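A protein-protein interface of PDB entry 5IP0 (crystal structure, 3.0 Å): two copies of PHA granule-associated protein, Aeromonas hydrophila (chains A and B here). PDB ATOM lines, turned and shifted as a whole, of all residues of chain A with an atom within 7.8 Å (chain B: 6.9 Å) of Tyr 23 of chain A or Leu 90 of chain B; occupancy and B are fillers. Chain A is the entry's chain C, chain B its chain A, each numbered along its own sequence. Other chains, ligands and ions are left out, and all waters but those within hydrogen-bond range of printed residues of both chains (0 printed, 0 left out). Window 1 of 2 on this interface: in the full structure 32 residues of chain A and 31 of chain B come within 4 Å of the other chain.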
ATOM      1  N   ALA A  17      21.933  -0.495  17.119  1.00  0.00           N
ATOM      2  CA  ALA A  17      23.197  -1.025  17.639  1.00  0.00           C
ATOM      3  C   ALA A  17      23.130  -2.551  17.650  1.00  0.00           C
ATOM      4  O   ALA A  17      22.583  -3.153  16.727  1.00  0.00           O
ATOM      5  CB  ALA A  17      23.482  -0.464  19.060  1.00  0.00           C
ATOM      6  N   ALA A  18      23.710  -3.163  18.684  1.00  0.00           N
ATOM      7  CA  ALA A  18      23.453  -4.556  19.022  1.00  0.00           C
ATOM      8  C   ALA A  18      24.115  -5.503  18.022  1.00  0.00           C
ATOM      9  O   ALA A  18      24.885  -5.063  17.142  1.00  0.00           O
ATOM     10  CB  ALA A  18      21.935  -4.783  19.113  1.00  0.00           C
ATOM     11  N   PRO A  19      23.879  -6.814  18.147  1.00  0.00           N
ATOM     12  CA  PRO A  19      24.427  -7.748  17.153  1.00  0.00           C
ATOM     13  C   PRO A  19      24.043  -7.453  15.716  1.00  0.00           C
ATOM     14  O   PRO A  19      24.743  -7.940  14.823  1.00  0.00           O
ATOM     15  CB  PRO A  19      23.901  -9.110  17.624  1.00  0.00           C
ATOM     16  CG  PRO A  19      23.890  -8.967  19.088  1.00  0.00           C
ATOM     17  CD  PRO A  19      23.479  -7.541  19.372  1.00  0.00           C
ATOM     18  N   LEU A  20      22.953  -6.736  15.438  1.00  0.00           N
ATOM     19  CA  LEU A  20      22.702  -6.354  14.048  1.00  0.00           C
ATOM     20  C   LEU A  20      23.939  -5.664  13.467  1.00  0.00           C
ATOM     21  O   LEU A  20      24.588  -6.161  12.528  1.00  0.00           O
ATOM     22  CB  LEU A  20      21.503  -5.408  13.952  1.00  0.00           C
ATOM     23  CG  LEU A  20      20.082  -5.927  14.125  1.00  0.00           C
ATOM     24  CD1 LEU A  20      19.780  -7.017  13.120  1.00  0.00           C
ATOM     25  CD2 LEU A  20      19.806  -6.370  15.533  1.00  0.00           C
ATOM     26  N   THR A  21      24.285  -4.513  14.052  1.00  0.00           N
ATOM     27  CA  THR A  21      25.508  -3.812  13.683  1.00  0.00           C
ATOM     28  C   THR A  21      26.704  -4.751  13.699  1.00  0.00           C
ATOM     29  O   THR A  21      27.440  -4.837  12.711  1.00  0.00           O
ATOM     30  CB  THR A  21      25.755  -2.631  14.632  1.00  0.00           C
ATOM     31  OG1 THR A  21      24.691  -1.674  14.528  1.00  0.00           O
ATOM     32  CG2 THR A  21      27.092  -1.956  14.336  1.00  0.00           C
ATOM     33  N   ARG A  22      26.869  -5.517  14.788  1.00  0.00           N
ATOM     34  CA  ARG A  22      28.021  -6.420  14.892  1.00  0.00           C
ATOM     35  C   ARG A  22      28.137  -7.347  13.672  1.00  0.00           C
ATOM     36  O   ARG A  22      29.240  -7.587  13.158  1.00  0.00           O
ATOM     37  CB  ARG A  22      27.904  -7.228  16.186  1.00  0.00           C
ATOM     38  CG  ARG A  22      29.213  -7.779  16.728  1.00  0.00           C
ATOM     39  CD  ARG A  22      29.949  -6.749  17.564  1.00  0.00           C
ATOM     40  NE  ARG A  22      31.269  -7.229  17.962  1.00  0.00           N
ATOM     41  CZ  ARG A  22      32.393  -6.950  17.308  1.00  0.00           C
ATOM     42  NH1 ARG A  22      32.360  -6.193  16.219  1.00  0.00           N
ATOM     43  NH2 ARG A  22      33.554  -7.421  17.739  1.00  0.00           N
ATOM     44  N   TYR A  23      26.997  -7.797  13.143  1.00  0.00           N
ATOM     45  CA  TYR A  23      26.946  -8.705  11.999  1.00  0.00           C
ATOM     46  C   TYR A  23      27.281  -8.004  10.686  1.00  0.00           C
ATOM     47  O   TYR A  23      28.029  -8.543   9.855  1.00  0.00           O
ATOM     48  CB  TYR A  23      25.559  -9.333  11.910  1.00  0.00           C
ATOM     49  CG  TYR A  23      25.288  -9.988  10.583  1.00  0.00           C
ATOM     50  CD1 TYR A  23      26.012 -11.100  10.201  1.00  0.00           C
ATOM     51  CD2 TYR A  23      24.301  -9.514   9.718  1.00  0.00           C
ATOM     52  CE1 TYR A  23      25.791 -11.716   9.006  1.00  0.00           C
ATOM     53  CE2 TYR A  23      24.066 -10.133   8.506  1.00  0.00           C
ATOM     54  CZ  TYR A  23      24.833 -11.236   8.158  1.00  0.00           C
ATOM     55  OH  TYR A  23      24.664 -11.906   6.972  1.00  0.00           O
ATOM     56  N   ASN A  24      26.714  -6.813  10.457  1.00  0.00           N
ATOM     57  CA  ASN A  24      27.093  -6.098   9.245  1.00  0.00           C
ATOM     58  C   ASN A  24      28.572  -5.745   9.262  1.00  0.00           C
ATOM     59  O   ASN A  24      29.245  -5.796   8.222  1.00  0.00           O
ATOM     60  CB  ASN A  24      26.202  -4.874   9.073  1.00  0.00           C
ATOM     61  CG  ASN A  24      24.766  -5.245   8.736  1.00  0.00           C
ATOM     62  OD1 ASN A  24      23.868  -5.067   9.545  1.00  0.00           O
ATOM     63  ND2 ASN A  24      24.546  -5.751   7.518  1.00  0.00           N
ATOM     64  N   GLN A  25      29.105  -5.472  10.449  1.00  0.00           N
ATOM     65  CA  GLN A  25      30.521  -5.155  10.589  1.00  0.00           C
ATOM     66  C   GLN A  25      31.400  -6.356  10.251  1.00  0.00           C
ATOM     67  O   GLN A  25      32.385  -6.223   9.528  1.00  0.00           O
ATOM     68  CB  GLN A  25      30.798  -4.678  12.009  1.00  0.00           C
ATOM     69  CG  GLN A  25      30.202  -3.324  12.324  1.00  0.00           C
ATOM     70  CD  GLN A  25      30.890  -2.211  11.584  1.00  0.00           C
ATOM     71  OE1 GLN A  25      32.040  -2.347  11.161  1.00  0.00           O
ATOM     72  NE2 GLN A  25      30.197  -1.087  11.434  1.00  0.00           N
ATOM     73  N   LEU A  26      31.092  -7.533  10.806  1.00  0.00           N
ATOM     74  CA  LEU A  26      31.833  -8.742  10.436  1.00  0.00           C
ATOM     75  C   LEU A  26      31.774  -9.008   8.935  1.00  0.00           C
ATOM     76  O   LEU A  26      32.782  -9.382   8.319  1.00  0.00           O
ATOM     77  CB  LEU A  26      31.296  -9.932  11.217  1.00  0.00           C
ATOM     78  CG  LEU A  26      31.981 -11.298  11.111  1.00  0.00           C
ATOM     79  CD1 LEU A  26      33.504 -11.263  11.170  1.00  0.00           C
ATOM     80  CD2 LEU A  26      31.388 -12.181  12.195  1.00  0.00           C
ATOM     81  N   LEU A  27      30.587  -8.849   8.336  1.00  0.00           N
ATOM     82  CA  LEU A  27      30.411  -9.017   6.890  1.00  0.00           C
ATOM     83  C   LEU A  27      31.384  -8.149   6.094  1.00  0.00           C
ATOM     84  O   LEU A  27      32.181  -8.638   5.272  1.00  0.00           O
ATOM     85  CB  LEU A  27      28.967  -8.648   6.522  1.00  0.00           C
ATOM     86  CG  LEU A  27      28.147  -9.489   5.553  1.00  0.00           C
ATOM     87  CD1 LEU A  27      28.500 -10.949   5.759  1.00  0.00           C
ATOM     88  CD2 LEU A  27      26.644  -9.244   5.777  1.00  0.00           C
ATOM     89  N   ALA A  28      31.302  -6.835   6.323  1.00  0.00           N
ATOM     90  CA  ALA A  28      32.153  -5.900   5.598  1.00  0.00           C
ATOM     91  C   ALA A  28      33.622  -6.157   5.908  1.00  0.00           C
ATOM     92  O   ALA A  28      34.482  -6.092   5.019  1.00  0.00           O
ATOM     93  CB  ALA A  28      31.747  -4.471   5.943  1.00  0.00           C
ATOM     94  N   SER A  29      33.912  -6.461   7.172  1.00  0.00           N
ATOM     95  CA  SER A  29      35.258  -6.805   7.612  1.00  0.00           C
ATOM     96  C   SER A  29      35.858  -7.892   6.740  1.00  0.00           C
ATOM     97  O   SER A  29      36.990  -7.767   6.246  1.00  0.00           O
ATOM     98  CB  SER A  29      35.197  -7.247   9.081  1.00  0.00           C
ATOM     99  OG  SER A  29      36.368  -7.923   9.502  1.00  0.00           O
ATOM    100  N   ASN A  30      35.100  -8.974   6.543  1.00  0.00           N
ATOM    101  CA  ASN A  30      35.605 -10.085   5.750  1.00  0.00           C
ATOM    102  C   ASN A  30      35.770  -9.688   4.292  1.00  0.00           C
ATOM    103  O   ASN A  30      36.771 -10.055   3.662  1.00  0.00           O
ATOM    104  CB  ASN A  30      34.687 -11.291   5.898  1.00  0.00           C
ATOM    105  CG  ASN A  30      34.893 -11.990   7.214  1.00  0.00           C
ATOM    106  OD1 ASN A  30      35.972 -12.520   7.484  1.00  0.00           O
ATOM    107  ND2 ASN A  30      33.888 -11.934   8.075  1.00  0.00           N
ATOM    108  N   MET A  83      37.584 -16.119  10.517  1.00  0.00           N
ATOM    109  CA  MET A  83      36.206 -15.801  10.172  1.00  0.00           C
ATOM    110  C   MET A  83      35.239 -16.744  10.869  1.00  0.00           C
ATOM    111  O   MET A  83      34.179 -16.315  11.342  1.00  0.00           O
ATOM    112  CB  MET A  83      35.988 -15.892   8.667  1.00  0.00           C
ATOM    113  CG  MET A  83      34.528 -15.606   8.254  1.00  0.00           C
ATOM    114  SD  MET A  83      34.210 -15.980   6.517  1.00  0.00           S
ATOM    115  CE  MET A  83      35.865 -15.693   5.859  1.00  0.00           C
ATOM    116  N   LEU A  84      35.585 -18.035  10.956  1.00  0.00           N
ATOM    117  CA  LEU A  84      34.670 -18.964  11.620  1.00  0.00           C
ATOM    118  C   LEU A  84      34.627 -18.753  13.134  1.00  0.00           C
ATOM    119  O   LEU A  84      33.566 -18.949  13.754  1.00  0.00           O
ATOM    120  CB  LEU A  84      35.013 -20.409  11.251  1.00  0.00           C
ATOM    121  CG  LEU A  84      34.420 -20.863   9.897  1.00  0.00           C
ATOM    122  CD1 LEU A  84      34.802 -22.288   9.555  1.00  0.00           C
ATOM    123  CD2 LEU A  84      32.896 -20.727   9.869  1.00  0.00           C
ATOM    124  N   ASP A  86      34.997 -15.746  14.612  1.00  0.00           N
ATOM    125  CA  ASP A  86      34.141 -14.576  14.770  1.00  0.00           C
ATOM    126  C   ASP A  86      32.689 -14.941  14.522  1.00  0.00           C
ATOM    127  O   ASP A  86      31.795 -14.399  15.175  1.00  0.00           O
ATOM    128  CB  ASP A  86      34.588 -13.425  13.848  1.00  0.00           C
ATOM    129  CG  ASP A  86      35.925 -12.792  14.280  1.00  0.00           C
ATOM    130  OD1 ASP A  86      36.285 -12.869  15.476  1.00  0.00           O
ATOM    131  OD2 ASP A  86      36.619 -12.206  13.418  1.00  0.00           O
ATOM    132  N   ILE A  87      32.430 -15.904  13.648  1.00  0.00           N
ATOM    133  CA  ILE A  87      31.043 -16.287  13.444  1.00  0.00           C
ATOM    134  C   ILE A  87      30.481 -16.933  14.708  1.00  0.00           C
ATOM    135  O   ILE A  87      29.362 -16.621  15.131  1.00  0.00           O
ATOM    136  CB  ILE A  87      30.923 -17.190  12.202  1.00  0.00           C
ATOM    137  CG1 ILE A  87      30.994 -16.324  10.947  1.00  0.00           C
ATOM    138  CG2 ILE A  87      29.595 -17.924  12.180  1.00  0.00           C
ATOM    139  CD1 ILE A  87      31.144 -17.105   9.663  1.00  0.00           C
ATOM    140  N   LEU A  90      29.878 -14.282  17.314  1.00  0.00           N
ATOM    141  CA  LEU A  90      28.744 -13.499  16.857  1.00  0.00           C
ATOM    142  C   LEU A  90      27.452 -14.217  17.172  1.00  0.00           C
ATOM    143  O   LEU A  90      26.501 -13.603  17.663  1.00  0.00           O
ATOM    144  CB  LEU A  90      28.853 -13.242  15.356  1.00  0.00           C
ATOM    145  CG  LEU A  90      27.689 -12.440  14.770  1.00  0.00           C
ATOM    146  CD1 LEU A  90      27.611 -11.083  15.442  1.00  0.00           C
ATOM    147  CD2 LEU A  90      27.835 -12.285  13.273  1.00  0.00           C
ATOM    148  N   LEU B  34      29.623 -12.645  -0.127  1.00  0.00           N
ATOM    149  CA  LEU B  34      29.542 -11.708   0.993  1.00  0.00           C
ATOM    150  C   LEU B  34      28.823 -10.410   0.605  1.00  0.00           C
ATOM    151  O   LEU B  34      27.976  -9.897   1.349  1.00  0.00           O
ATOM    152  CB  LEU B  34      30.945 -11.396   1.485  1.00  0.00           C
ATOM    153  CG  LEU B  34      31.615 -12.540   2.205  1.00  0.00           C
ATOM    154  CD1 LEU B  34      33.067 -12.242   2.420  1.00  0.00           C
ATOM    155  CD2 LEU B  34      30.938 -12.734   3.538  1.00  0.00           C
ATOM    156  N   LEU B  37      25.143 -11.055   0.436  1.00  0.00           N
ATOM    157  CA  LEU B  37      24.606 -11.122   1.795  1.00  0.00           C
ATOM    158  C   LEU B  37      24.386  -9.743   2.407  1.00  0.00           C
ATOM    159  O   LEU B  37      23.354  -9.503   3.042  1.00  0.00           O
ATOM    160  CB  LEU B  37      25.546 -11.923   2.690  1.00  0.00           C
ATOM    161  CG  LEU B  37      25.228 -13.382   2.947  1.00  0.00           C
ATOM    162  CD1 LEU B  37      26.258 -13.931   3.879  1.00  0.00           C
ATOM    163  CD2 LEU B  37      23.857 -13.422   3.596  1.00  0.00           C
ATOM    164  N   GLN B  38      25.359  -8.832   2.253  1.00  0.00           N
ATOM    165  CA  GLN B  38      25.221  -7.477   2.798  1.00  0.00           C
ATOM    166  C   GLN B  38      24.061  -6.729   2.135  1.00  0.00           C
ATOM    167  O   GLN B  38      23.326  -5.986   2.802  1.00  0.00           O
ATOM    168  CB  GLN B  38      26.539  -6.713   2.647  1.00  0.00           C
ATOM    169  CG  GLN B  38      26.603  -5.374   3.383  1.00  0.00           C
ATOM    170  CD  GLN B  38      26.823  -5.490   4.885  1.00  0.00           C
ATOM    171  OE1 GLN B  38      25.888  -5.756   5.647  1.00  0.00           O
ATOM    172  NE2 GLN B  38      28.055  -5.212   5.325  1.00  0.00           N
ATOM    173  N   SER B  41      20.807  -8.197   3.629  1.00  0.00           N
ATOM    174  CA  SER B  41      20.590  -7.654   4.972  1.00  0.00           C
ATOM    175  C   SER B  41      20.104  -6.217   4.905  1.00  0.00           C
ATOM    176  O   SER B  41      19.106  -5.853   5.540  1.00  0.00           O
ATOM    177  CB  SER B  41      21.873  -7.711   5.807  1.00  0.00           C
ATOM    178  OG  SER B  41      22.262  -9.035   6.097  1.00  0.00           O
ATOM    179  N   TYR B  45      16.565  -4.757   6.473  1.00  0.00           N
ATOM    180  CA  TYR B  45      16.392  -3.690   7.459  1.00  0.00           C
ATOM    181  C   TYR B  45      15.612  -2.508   6.880  1.00  0.00           C
ATOM    182  O   TYR B  45      14.780  -1.901   7.571  1.00  0.00           O
ATOM    183  CB  TYR B  45      17.748  -3.212   7.965  1.00  0.00           C
ATOM    184  CG  TYR B  45      18.646  -4.231   8.619  1.00  0.00           C
ATOM    185  CD1 TYR B  45      18.132  -5.280   9.376  1.00  0.00           C
ATOM    186  CD2 TYR B  45      20.028  -4.117   8.502  1.00  0.00           C
ATOM    187  CE1 TYR B  45      18.986  -6.195   9.990  1.00  0.00           C
ATOM    188  CE2 TYR B  45      20.884  -5.012   9.104  1.00  0.00           C
ATOM    189  CZ  TYR B  45      20.375  -6.049   9.854  1.00  0.00           C
ATOM    190  OH  TYR B  45      21.273  -6.928  10.445  1.00  0.00           O
ATOM    191  N   GLN B  82      15.072 -12.541  10.611  1.00  0.00           N
ATOM    192  CA  GLN B  82      16.082 -12.102   9.653  1.00  0.00           C
ATOM    193  C   GLN B  82      17.480 -12.176  10.247  1.00  0.00           C
ATOM    194  O   GLN B  82      18.441 -12.545   9.561  1.00  0.00           O
ATOM    195  CB  GLN B  82      15.769 -10.680   9.193  1.00  0.00           C
ATOM    196  CG  GLN B  82      15.807 -10.522   7.684  1.00  0.00           C
ATOM    197  CD  GLN B  82      17.217 -10.507   7.157  1.00  0.00           C
ATOM    198  OE1 GLN B  82      17.553 -11.207   6.196  1.00  0.00           O
ATOM    199  NE2 GLN B  82      18.063  -9.685   7.784  1.00  0.00           N
ATOM    200  N   MET B  83      17.604 -11.862  11.531  1.00  0.00           N
ATOM    201  CA  MET B  83      18.915 -11.835  12.158  1.00  0.00           C
ATOM    202  C   MET B  83      19.515 -13.224  12.260  1.00  0.00           C
ATOM    203  O   MET B  83      20.693 -13.441  11.931  1.00  0.00           O
ATOM    204  CB  MET B  83      18.794 -11.220  13.537  1.00  0.00           C
ATOM    205  CG  MET B  83      19.868 -11.663  14.456  1.00  0.00           C
ATOM    206  SD  MET B  83      19.625 -10.782  15.983  1.00  0.00           S
ATOM    207  CE  MET B  83      20.085 -12.064  17.109  1.00  0.00           C
ATOM    208  N   LEU B  84      18.710 -14.187  12.700  1.00  0.00           N
ATOM    209  CA  LEU B  84      19.213 -15.548  12.808  1.00  0.00           C
ATOM    210  C   LEU B  84      19.489 -16.154  11.426  1.00  0.00           C
ATOM    211  O   LEU B  84      20.546 -16.765  11.207  1.00  0.00           O
ATOM    212  CB  LEU B  84      18.225 -16.368  13.622  1.00  0.00           C
ATOM    213  CG  LEU B  84      18.291 -15.956  15.101  1.00  0.00           C
ATOM    214  CD1 LEU B  84      17.184 -16.616  15.940  1.00  0.00           C
ATOM    215  CD2 LEU B  84      19.677 -16.207  15.686  1.00  0.00           C
ATOM    216  N   ASP B  85      18.579 -15.951  10.462  1.00  0.00           N
ATOM    217  CA  ASP B  85      18.803 -16.518   9.135  1.00  0.00           C
ATOM    218  C   ASP B  85      20.043 -15.912   8.488  1.00  0.00           C
ATOM    219  O   ASP B  85      20.783 -16.616   7.794  1.00  0.00           O
ATOM    220  CB  ASP B  85      17.565 -16.343   8.252  1.00  0.00           C
ATOM    221  CG  ASP B  85      17.533 -17.320   7.049  1.00  0.00           C
ATOM    222  OD1 ASP B  85      18.319 -18.301   6.984  1.00  0.00           O
ATOM    223  OD2 ASP B  85      16.676 -17.123   6.167  1.00  0.00           O
ATOM    224  N   ASP B  86      20.287 -14.608   8.708  1.00  0.00           N
ATOM    225  CA  ASP B  86      21.509 -13.966   8.217  1.00  0.00           C
ATOM    226  C   ASP B  86      22.753 -14.608   8.821  1.00  0.00           C
ATOM    227  O   ASP B  86      23.722 -14.907   8.109  1.00  0.00           O
ATOM    228  CB  ASP B  86      21.507 -12.463   8.532  1.00  0.00           C
ATOM    229  CG  ASP B  86      20.808 -11.616   7.478  1.00  0.00           C
ATOM    230  OD1 ASP B  86      20.441 -12.162   6.410  1.00  0.00           O
ATOM    231  OD2 ASP B  86      20.697 -10.376   7.708  1.00  0.00           O
ATOM    232  N   ILE B  87      22.757 -14.806  10.146  1.00  0.00           N
ATOM    233  CA  ILE B  87      23.910 -15.457  10.772  1.00  0.00           C
ATOM    234  C   ILE B  87      24.130 -16.844  10.175  1.00  0.00           C
ATOM    235  O   ILE B  87      25.268 -17.260   9.922  1.00  0.00           O
ATOM    236  CB  ILE B  87      23.730 -15.547  12.298  1.00  0.00           C
ATOM    237  CG1 ILE B  87      23.551 -14.161  12.893  1.00  0.00           C
ATOM    238  CG2 ILE B  87      24.961 -16.185  12.928  1.00  0.00           C
ATOM    239  CD1 ILE B  87      23.428 -14.164  14.387  1.00  0.00           C
ATOM    240  N   GLN B  88      23.049 -17.590   9.948  1.00  0.00           N
ATOM    241  CA  GLN B  88      23.213 -18.938   9.419  1.00  0.00           C
ATOM    242  C   GLN B  88      23.794 -18.906   8.007  1.00  0.00           C
ATOM    243  O   GLN B  88      24.799 -19.568   7.726  1.00  0.00           O
ATOM    244  CB  GLN B  88      21.880 -19.683   9.474  1.00  0.00           C
ATOM    245  CG  GLN B  88      22.010 -21.202   9.378  1.00  0.00           C
ATOM    246  CD  GLN B  88      22.142 -21.684   7.942  1.00  0.00           C
ATOM    247  OE1 GLN B  88      21.827 -20.949   6.994  1.00  0.00           O
ATOM    248  NE2 GLN B  88      22.611 -22.920   7.769  1.00  0.00           N
ATOM    249  N   LYS B  89      23.178 -18.126   7.111  1.00  0.00           N
ATOM    250  CA  LYS B  89      23.746 -17.875   5.786  1.00  0.00           C
ATOM    251  C   LYS B  89      25.243 -17.608   5.864  1.00  0.00           C
ATOM    252  O   LYS B  89      26.040 -18.214   5.133  1.00  0.00           O
ATOM    253  CB  LYS B  89      23.040 -16.675   5.152  1.00  0.00           C
ATOM    254  CG  LYS B  89      21.661 -16.963   4.649  1.00  0.00           C
ATOM    255  CD  LYS B  89      20.898 -15.690   4.369  1.00  0.00           C
ATOM    256  CE  LYS B  89      19.651 -15.944   3.538  1.00  0.00           C
ATOM    257  NZ  LYS B  89      19.031 -14.638   3.146  1.00  0.00           N
ATOM    258  N   LEU B  90      25.650 -16.702   6.760  1.00  0.00           N
ATOM    259  CA  LEU B  90      27.067 -16.378   6.855  1.00  0.00           C
ATOM    260  C   LEU B  90      27.891 -17.575   7.295  1.00  0.00           C
ATOM    261  O   LEU B  90      28.944 -17.852   6.712  1.00  0.00           O
ATOM    262  CB  LEU B  90      27.285 -15.205   7.797  1.00  0.00           C
ATOM    263  CG  LEU B  90      28.752 -14.816   7.836  1.00  0.00           C
ATOM    264  CD1 LEU B  90      29.293 -14.685   6.445  1.00  0.00           C
ATOM    265  CD2 LEU B  90      28.819 -13.483   8.497  1.00  0.00           C
ATOM    266  N   SER B  91      27.408 -18.323   8.291  1.00  0.00           N
ATOM    267  CA  SER B  91      28.140 -19.504   8.735  1.00  0.00           C
ATOM    268  C   SER B  91      28.330 -20.481   7.584  1.00  0.00           C
ATOM    269  O   SER B  91      29.437 -20.986   7.364  1.00  0.00           O
ATOM    270  CB  SER B  91      27.418 -20.180   9.897  1.00  0.00           C
ATOM    271  OG  SER B  91      28.219 -21.226  10.431  1.00  0.00           O
ATOM    272  N   ALA B  92      27.280 -20.698   6.793  1.00  0.00           N
ATOM    273  CA  ALA B  92      27.396 -21.580   5.645  1.00  0.00           C
ATOM    274  C   ALA B  92      28.481 -21.095   4.709  1.00  0.00           C
ATOM    275  O   ALA B  92      29.356 -21.860   4.287  1.00  0.00           O
ATOM    276  CB  ALA B  92      26.065 -21.638   4.913  1.00  0.00           C
ATOM    277  N   LEU B  93      28.470 -19.800   4.431  1.00  0.00           N
ATOM    278  CA  LEU B  93      29.458 -19.229   3.528  1.00  0.00           C
ATOM    279  C   LEU B  93      30.869 -19.487   4.031  1.00  0.00           C
ATOM    280  O   LEU B  93      31.763 -19.867   3.253  1.00  0.00           O
ATOM    281  CB  LEU B  93      29.153 -17.753   3.379  1.00  0.00           C
ATOM    282  CG  LEU B  93      29.786 -17.024   2.239  1.00  0.00           C
ATOM    283  CD1 LEU B  93      28.744 -16.000   1.911  1.00  0.00           C
ATOM    284  CD2 LEU B  93      31.088 -16.381   2.728  1.00  0.00           C
ATOM    285  N   GLY B  94      31.063 -19.341   5.347  1.00  0.00           N
ATOM    286  CA  GLY B  94      32.366 -19.581   5.937  1.00  0.00           C
ATOM    287  C   GLY B  94      32.785 -21.033   5.866  1.00  0.00           C
ATOM    288  O   GLY B  94      33.944 -21.340   5.565  1.00  0.00           O
ATOM    289  N   GLN B  95      31.846 -21.948   6.128  1.00  0.00           N
ATOM    290  CA  GLN B  95      32.122 -23.377   5.986  1.00  0.00           C
ATOM    291  C   GLN B  95      32.543 -23.717   4.561  1.00  0.00           C
ATOM    292  O   GLN B  95      33.634 -24.241   4.327  1.00  0.00           O
ATOM    293  CB  GLN B  95      30.900 -24.209   6.382  1.00  0.00           C
ATOM    294  CG  GLN B  95      30.432 -24.133   7.850  1.00  0.00           C
ATOM    295  CD  GLN B  95      31.401 -24.747   8.849  1.00  0.00           C
ATOM    296  OE1 GLN B  95      32.296 -25.514   8.482  1.00  0.00           O
ATOM    297  NE2 GLN B  95      31.191 -24.452  10.135  1.00  0.00           N
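OD1 of Asn 24 of chain A lies close to O of Leu 20 of chain A (3.3 Å).
The backbone carbonyl oxygen (O) of Leu 37 of chain B is in hydrogen-bond range of the side-chain hydroxyl (OG) of Ser 41 of chain B (3.3 Å).
NE2 of Gln 82 of chain B lies within hydrogen-bond range of OD2 of Asp 86 of chain B (2.7 Å).
The backbone carbonyl oxygen of Leu 26 of chain A is in hydrogen-bond range of the side-chain amide nitrogen of Asn 30 of chain A, 2.8 Å away.
OG of Ser 41 of chain B lies within hydrogen-bond range of OD2 of Asp 86 of chain B.
Ile 87 of chain A touches Leu 90 of chain B, but with the chains exchanged Leu 90 of chain A does not touch Ile 87 of chain B (4.5 Å).
Of the 19 printed residues of chain A, 7 touch a printed residue of chain B.
Printed residues of chain A that touch a printed residue of chain B: Leu 20, Tyr 23, Asn 24, Leu 27, Ala 28, Asn 30 and Ile 87.
Hydrophobic or aromatic side chains of chain A that line the printed part of chain B: Leu 20, Tyr 23, Leu 27, Ala 28 and Ile 87.
Of the 19 printed residues of chain B, 8 touch a printed residue of chain A.
Of chain A, only Tyr 23 (3.5 Å), Leu 27 (3.7 Å) and Ile 87 (3.8 Å) come within 4 Å of Leu 90 of chain B.
Printed residues of chain A within 4 Å of Ser 91 of chain B: Ile 87 (3.9 Å).
Of the printed residues of chain B, Leu 27 of chain A touches Leu 34 (3.8 Å), Gln 38 (3.6 Å) and Leu 90 (3.7 Å).
Of the printed residues of chain B, Ala 28 of chain A touches Gln 38.
The nearest residue of chain B that does not touch Tyr 23 of chain A is Tyr 45 of chain B (4.05 Å).
The nearest residue of chain A that does not touch Leu 90 of chain B is Leu 26 of chain A (4.6 Å).
Among the printed residues, pairs that only touch across the chains: Leu 20 of chain A with Tyr 45 of chain B (3.1 Å), Tyr 23 of chain A with Leu 37 of chain B (3.8 Å), Tyr 23 of chain A with Ser 41 of chain B (3.2 Å), Tyr 23 of chain A with Leu 90 of chain B (3.5 Å), Asn 24 of chain A with Ser 41 of chain B (3.7 Å), Leu 27 of chain A with Leu 34 of chain B (3.8 Å), Leu 27 of chain A with Gln 38 of chain B (3.6 Å), Leu 27 of chain A with Leu 90 of chain B (3.7 Å), Ala 28 of chain A with Gln 38 of chain B (3.8 Å), Asn 30 of chain A with Leu 34 of chain B (3.95 Å), Ile 87 of chain A with Leu 90 of chain B (3.8 Å) and Ile 87 of chain A with Ser 91 of chain B (3.9 Å).
The backbone carbonyl oxygen (O) of Asp 86 of chain B lies within hydrogen-bond range of the side-chain hydroxyl (OH) of Tyr 23 of chain A.
The side-chain amide oxygen (OD1) of Asn 24 of chain A sits close to the side-chain hydroxyl (OH) of Tyr 45 of chain B (3.3 Å).
O of Asn 24 of chain A lies within hydrogen-bond range of NE2 of Gln 38 of chain B (3.2 Å).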
